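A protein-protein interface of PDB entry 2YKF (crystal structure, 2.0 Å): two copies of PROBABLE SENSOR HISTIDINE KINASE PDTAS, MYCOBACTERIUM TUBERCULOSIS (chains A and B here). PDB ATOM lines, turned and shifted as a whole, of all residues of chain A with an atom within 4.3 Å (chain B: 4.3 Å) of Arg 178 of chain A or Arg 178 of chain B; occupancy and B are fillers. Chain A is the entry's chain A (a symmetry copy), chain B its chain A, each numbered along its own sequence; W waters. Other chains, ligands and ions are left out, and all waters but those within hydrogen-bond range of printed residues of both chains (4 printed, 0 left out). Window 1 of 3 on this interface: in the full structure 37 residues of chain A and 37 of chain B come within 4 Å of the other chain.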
ATOM      1  N   ASN A  62     -23.673 -20.070 -10.794  1.00  0.00           N
ATOM      2  CA  ASN A  62     -23.019 -20.650 -11.949  1.00  0.00           C
ATOM      3  C   ASN A  62     -23.121 -22.146 -11.991  1.00  0.00           C
ATOM      4  O   ASN A  62     -22.790 -22.717 -13.010  1.00  0.00           O
ATOM      5  CB  ASN A  62     -21.539 -20.229 -12.007  1.00  0.00           C
ATOM      6  CG  ASN A  62     -21.403 -18.755 -12.453  1.00  0.00           C
ATOM      7  OD1 ASN A  62     -22.321 -18.198 -13.061  1.00  0.00           O
ATOM      8  ND2 ASN A  62     -20.292 -18.160 -12.191  1.00  0.00           N
ATOM      9  N   SER A 176      -9.445 -16.165  -7.399  1.00  0.00           N
ATOM     10  CA  SER A 176      -9.593 -17.246  -6.417  1.00  0.00           C
ATOM     11  C   SER A 176     -10.484 -18.352  -6.977  1.00  0.00           C
ATOM     12  O   SER A 176     -11.292 -18.080  -7.844  1.00  0.00           O
ATOM     13  CB  SER A 176     -10.133 -16.760  -5.094  1.00  0.00           C
ATOM     14  OG  SER A 176     -11.396 -16.191  -5.268  1.00  0.00           O
ATOM     15  N   PRO A 177     -10.350 -19.572  -6.448  1.00  0.00           N
ATOM     16  CA  PRO A 177     -11.152 -20.728  -6.933  1.00  0.00           C
ATOM     17  C   PRO A 177     -12.646 -20.433  -6.831  1.00  0.00           C
ATOM     18  O   PRO A 177     -13.031 -19.708  -5.928  1.00  0.00           O
ATOM     19  CB  PRO A 177     -10.829 -21.838  -5.934  1.00  0.00           C
ATOM     20  CG  PRO A 177      -9.725 -21.387  -5.138  1.00  0.00           C
ATOM     21  CD  PRO A 177      -9.564 -19.884  -5.251  1.00  0.00           C
ATOM     22  N   ARG A 178     -13.452 -20.930  -7.762  1.00  0.00           N
ATOM     23  CA  ARG A 178     -14.878 -20.974  -7.608  1.00  0.00           C
ATOM     24  C   ARG A 178     -15.177 -22.272  -6.875  1.00  0.00           C
ATOM     25  O   ARG A 178     -14.384 -23.198  -6.875  1.00  0.00           O
ATOM     26  CB  ARG A 178     -15.595 -20.943  -8.991  1.00  0.00           C
ATOM     27  CG  ARG A 178     -15.065 -19.825  -9.976  1.00  0.00           C
ATOM     28  CD  ARG A 178     -15.306 -18.379  -9.443  1.00  0.00           C
ATOM     29  NE  ARG A 178     -14.910 -17.396 -10.480  1.00  0.00           N
ATOM     30  CZ  ARG A 178     -15.755 -16.860 -11.369  1.00  0.00           C
ATOM     31  NH1 ARG A 178     -17.059 -17.180 -11.357  1.00  0.00           N
ATOM     32  NH2 ARG A 178     -15.312 -15.980 -12.279  1.00  0.00           N
ATOM     33  N   ALA A 179     -16.305 -22.319  -6.176  1.00  0.00           N
ATOM     34  CA  ALA A 179     -16.739 -23.570  -5.532  1.00  0.00           C
ATOM     35  C   ALA A 179     -16.596 -24.823  -6.454  1.00  0.00           C
ATOM     36  O   ALA A 179     -16.031 -25.850  -6.049  1.00  0.00           O
ATOM     37  CB  ALA A 179     -18.219 -23.392  -5.020  1.00  0.00           C
ATOM     38  N   GLY A 180     -17.058 -24.735  -7.701  1.00  0.00           N
ATOM     39  CA  GLY A 180     -16.945 -25.892  -8.585  1.00  0.00           C
ATOM     40  C   GLY A 180     -15.541 -26.370  -8.867  1.00  0.00           C
ATOM     41  O   GLY A 180     -15.338 -27.565  -9.212  1.00  0.00           O
ATOM     42  N   ASP A 181     -14.562 -25.454  -8.783  1.00  0.00           N
ATOM     43  CA  ASP A 181     -13.155 -25.839  -8.969  1.00  0.00           C
ATOM     44  C   ASP A 181     -12.666 -26.924  -8.012  1.00  0.00           C
ATOM     45  O   ASP A 181     -11.751 -27.691  -8.346  1.00  0.00           O
ATOM     46  CB  ASP A 181     -12.221 -24.600  -8.894  1.00  0.00           C
ATOM     47  CG  ASP A 181     -12.522 -23.569 -10.007  1.00  0.00           C
ATOM     48  OD1 ASP A 181     -13.014 -23.943 -11.118  1.00  0.00           O
ATOM     49  OD2 ASP A 181     -12.269 -22.367  -9.790  1.00  0.00           O
ATOM     50  N   GLY A 182     -13.167 -26.925  -6.771  1.00  0.00           N
ATOM     51  CA  GLY A 182     -12.694 -27.921  -5.798  1.00  0.00           C
ATOM     52  C   GLY A 182     -13.158 -27.428  -4.407  1.00  0.00           C
ATOM     53  O   GLY A 182     -12.937 -26.271  -4.050  1.00  0.00           O
ATOM     54  N   ARG A 281      -8.227 -24.755  -6.629  1.00  0.00           N
ATOM     55  CA  ARG A 281      -8.327 -24.815  -8.078  1.00  0.00           C
ATOM     56  C   ARG A 281      -6.955 -25.262  -8.587  1.00  0.00           C
ATOM     57  O   ARG A 281      -5.969 -24.621  -8.269  1.00  0.00           O
ATOM     58  CB  ARG A 281      -8.608 -23.435  -8.665  1.00  0.00           C
ATOM     59  CG  ARG A 281      -8.753 -23.550 -10.206  1.00  0.00           C
ATOM     60  CD  ARG A 281      -8.964 -22.227 -10.966  1.00  0.00           C
ATOM     61  NE  ARG A 281      -9.340 -22.642 -12.329  1.00  0.00           N
ATOM     62  CZ  ARG A 281      -9.319 -21.863 -13.426  1.00  0.00           C
ATOM     63  NH1 ARG A 281      -9.012 -20.554 -13.332  1.00  0.00           N
ATOM     64  NH2 ARG A 281      -9.712 -22.392 -14.606  1.00  0.00           N
ATOM     65  N   ASN B  62     -18.354 -27.033 -14.403  1.00  0.00           N
ATOM     66  CA  ASN B  62     -18.823 -26.320 -13.233  1.00  0.00           C
ATOM     67  C   ASN B  62     -20.273 -25.944 -13.317  1.00  0.00           C
ATOM     68  O   ASN B  62     -20.818 -25.528 -12.315  1.00  0.00           O
ATOM     69  CB  ASN B  62     -17.973 -25.059 -12.986  1.00  0.00           C
ATOM     70  CG  ASN B  62     -16.586 -25.434 -12.416  1.00  0.00           C
ATOM     71  OD1 ASN B  62     -16.408 -26.525 -11.869  1.00  0.00           O
ATOM     72  ND2 ASN B  62     -15.652 -24.553 -12.513  1.00  0.00           N
ATOM     73  N   SER B 176      -9.902 -14.569 -15.958  1.00  0.00           N
ATOM     74  CA  SER B 176     -10.865 -14.291 -17.030  1.00  0.00           C
ATOM     75  C   SER B 176     -12.246 -14.823 -16.654  1.00  0.00           C
ATOM     76  O   SER B 176     -12.330 -15.741 -15.860  1.00  0.00           O
ATOM     77  CB  SER B 176     -10.432 -14.854 -18.362  1.00  0.00           C
ATOM     78  OG  SER B 176     -10.304 -16.242 -18.280  1.00  0.00           O
ATOM     79  N   PRO B 177     -13.301 -14.269 -17.258  1.00  0.00           N
ATOM     80  CA  PRO B 177     -14.692 -14.696 -16.951  1.00  0.00           C
ATOM     81  C   PRO B 177     -14.865 -16.194 -17.188  1.00  0.00           C
ATOM     82  O   PRO B 177     -14.203 -16.720 -18.069  1.00  0.00           O
ATOM     83  CB  PRO B 177     -15.535 -13.961 -17.993  1.00  0.00           C
ATOM     84  CG  PRO B 177     -14.683 -13.001 -18.630  1.00  0.00           C
ATOM     85  CD  PRO B 177     -13.225 -13.335 -18.386  1.00  0.00           C
ATOM     86  N   ARG B 178     -15.683 -16.869 -16.389  1.00  0.00           N
ATOM     87  CA  ARG B 178     -16.149 -18.191 -16.697  1.00  0.00           C
ATOM     88  C   ARG B 178     -17.391 -18.005 -17.555  1.00  0.00           C
ATOM     89  O   ARG B 178     -18.021 -16.961 -17.541  1.00  0.00           O
ATOM     90  CB  ARG B 178     -16.489 -18.985 -15.399  1.00  0.00           C
ATOM     91  CG  ARG B 178     -15.373 -18.915 -14.281  1.00  0.00           C
ATOM     92  CD  ARG B 178     -14.024 -19.561 -14.724  1.00  0.00           C
ATOM     93  NE  ARG B 178     -13.083 -19.579 -13.579  1.00  0.00           N
ATOM     94  CZ  ARG B 178     -12.933 -20.616 -12.746  1.00  0.00           C
ATOM     95  NH1 ARG B 178     -13.637 -21.746 -12.920  1.00  0.00           N
ATOM     96  NH2 ARG B 178     -12.060 -20.547 -11.730  1.00  0.00           N
ATOM     97  N   ALA B 179     -17.710 -19.002 -18.371  1.00  0.00           N
ATOM     98  CA  ALA B 179     -18.957 -18.965 -19.151  1.00  0.00           C
ATOM     99  C   ALA B 179     -20.196 -18.502 -18.319  1.00  0.00           C
ATOM    100  O   ALA B 179     -20.948 -17.610 -18.739  1.00  0.00           O
ATOM    101  CB  ALA B 179     -19.193 -20.380 -19.802  1.00  0.00           C
ATOM    102  N   GLY B 180     -20.388 -19.062 -17.124  1.00  0.00           N
ATOM    103  CA  GLY B 180     -21.540 -18.655 -16.325  1.00  0.00           C
ATOM    104  C   GLY B 180     -21.587 -17.198 -15.932  1.00  0.00           C
ATOM    105  O   GLY B 180     -22.690 -16.652 -15.661  1.00  0.00           O
ATOM    106  N   ASP B 181     -20.410 -16.558 -15.841  1.00  0.00           N
ATOM    107  CA  ASP B 181     -20.359 -15.119 -15.537  1.00  0.00           C
ATOM    108  C   ASP B 181     -21.131 -14.239 -16.517  1.00  0.00           C
ATOM    109  O   ASP B 181     -21.608 -13.157 -16.148  1.00  0.00           O
ATOM    110  CB  ASP B 181     -18.891 -14.625 -15.418  1.00  0.00           C
ATOM    111  CG  ASP B 181     -18.128 -15.323 -14.267  1.00  0.00           C
ATOM    112  OD1 ASP B 181     -18.751 -15.755 -13.246  1.00  0.00           O
ATOM    113  OD2 ASP B 181     -16.891 -15.450 -14.363  1.00  0.00           O
ATOM    114  N   GLY B 182     -21.155 -14.617 -17.801  1.00  0.00           N
ATOM    115  CA  GLY B 182     -21.847 -13.779 -18.792  1.00  0.00           C
ATOM    116  C   GLY B 182     -21.376 -14.268 -20.182  1.00  0.00           C
ATOM    117  O   GLY B 182     -20.177 -14.399 -20.424  1.00  0.00           O
ATOM    118  N   ARG B 281     -17.561 -10.629 -17.251  1.00  0.00           N
ATOM    119  CA  ARG B 281     -17.802 -10.814 -15.830  1.00  0.00           C
ATOM    120  C   ARG B 281     -17.855  -9.415 -15.214  1.00  0.00           C
ATOM    121  O   ARG B 281     -16.910  -8.663 -15.375  1.00  0.00           O
ATOM    122  CB  ARG B 281     -16.647 -11.564 -15.171  1.00  0.00           C
ATOM    123  CG  ARG B 281     -16.965 -11.783 -13.669  1.00  0.00           C
ATOM    124  CD  ARG B 281     -15.861 -12.461 -12.835  1.00  0.00           C
ATOM    125  NE  ARG B 281     -16.514 -12.789 -11.556  1.00  0.00           N
ATOM    126  CZ  ARG B 281     -15.887 -13.101 -10.406  1.00  0.00           C
ATOM    127  NH1 ARG B 281     -14.545 -13.220 -10.367  1.00  0.00           N
ATOM    128  NH2 ARG B 281     -16.634 -13.394  -9.319  1.00  0.00           N
HETATM  129  O   HOH W   1      -9.124 -19.108 -11.066  1.00  0.00           O
HETATM  130  O   HOH W   2     -20.011 -22.599 -13.968  1.00  0.00           O
HETATM  131  O   HOH W   3     -19.949 -23.012 -11.061  1.00  0.00           O
HETATM  132  O   HOH W   4     -12.974 -13.612 -12.514  1.00  0.00           O
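The side-chain amide oxygen of Asn 62 of chain B sits close to the backbone carbonyl oxygen of Gly 180 of chain A, 3.0 Å away. ND2 of Asn 62 of chain B is in hydrogen-bond range of OD1 of Asp 181 of chain A, at 3.0 Å. OD2 of Asp 181 of chain B is in salt-bridge range of NH2 of Arg 178 of chain A (2.7 Å). The guanidinium group (NH2) of Arg 178 of chain A lies close to the guanidinium group (NH1) of Arg 281 of chain B, at 3.4 Å. The guanidinium group (NH1) of Arg 281 of chain A lies close to the guanidinium group (NH2) of Arg 178 of chain B, 3.4 Å away. O of Gly 180 of chain B sits close to OD1 of Asn 62 of chain A (3.0 Å). The side-chain carboxylate (OD1) of Asp 181 of chain B sits at hydrogen-bond distance from the side-chain amide nitrogen (ND2) of Asn 62 of chain A, at 3.0 Å. NH2 of Arg 178 of chain B is in salt-bridge range of OD2 of Asp 181 of chain A, 2.7 Å away.
N of Arg 178 of chain B sits at hydrogen-bond distance from OD2 of Asp 181 of chain B (2.8 Å). The side-chain amide nitrogen (ND2) of Asn 62 of chain B lies close to the guanidinium group (NH1) of Arg 178 of chain B, at 3.5 Å. OD2 of Asp 181 of chain A is in salt-bridge range of NE of Arg 281 of chain A (3.9 Å). The side-chain carboxylate (OD2) of Asp 181 of chain B is in salt-bridge range of the guanidinium group (NE) of Arg 281 of chain B (3.9 Å). NH1 of Arg 178 of chain A sits close to ND2 of Asn 62 of chain A (3.5 Å). The backbone NH (N) of Arg 178 of chain A sits at hydrogen-bond distance from the side-chain carboxylate (OD2) of Asp 181 of chain A.
Among the printed residues, pairs that only touch across the chains: Asn 62 of chain A with Asn 62 of chain B and Arg 178 of chain A with Arg 178 of chain B.
Of chain B, only Arg 178 (3.6 Å), Asp 181 (2.7 Å) and Arg 281 (3.4 Å) come within 4 Å of Arg 178 of chain A. Arg 178 of chain B touches three residues of chain A. Of the printed residues of chain B, Arg 281 of chain A touches Arg 178. Printed residues of chain A within 4 Å of Gly 180 of chain B: Asn 62. Pro 177 of chain A touches none of the printed residues of chain B. Ser 176 of chain B touches none of the printed residues of chain A.
Of the 9 printed residues of chain B, 5 touch a printed residue of chain A. Printed residues of chain A that touch a printed residue of chain B: Asn 62, Arg 178, Gly 180, Asp 181 and Arg 281. Among the printed residues, 10 pairs touch across the chains. Among the printed residues, Asp or Glu carboxylates within 4 Å of a Lys or Arg side-chain nitrogen of the other chain: Arg 178 of chain A with Asp 181 of chain B and Asp 181 of chain A with Arg 178 of chain B.
Asn 62 of chain A touches its own counterpart, Asn 62 of chain B. Asn 62 of chain A touches Gly 180 of chain B, and with the chains exchanged Gly 180 of chain A touches Asn 62 of chain B. Arg 178 of chain A touches its own counterpart, Arg 178 of chain B. Arg 178 of chain A touches Arg 281 of chain B, and with the chains exchanged Arg 281 of chain A touches Arg 178 of chain B. 9 positions are printed for both chains. Of the 10 pairs that touch across the chains among the printed residues, 10 have their exchanged pair printed and touching as well.
Water W4 bridges the guanidinium group (NH1) of Arg 281 of chain B (2.7 Å) and the guanidinium group (NH2) of Arg 178 of chain A (3.3 Å). Water W1 lies within hydrogen-bond range of NH1 of Arg 281 of chain A and NH2 of Arg 178 of chain B. Water W3 bridges the backbone carbonyl oxygen (O) of Asn 62 of chain B (2.9 Å) and the backbone carbonyl oxygen (O) of Asn 62 of chain A (3.5 Å). Water W2 bridges the backbone carbonyl oxygen of Asn 62 of chain A (2.9 Å) and the backbone carbonyl oxygen of Asn 62 of chain B (3.5 Å).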
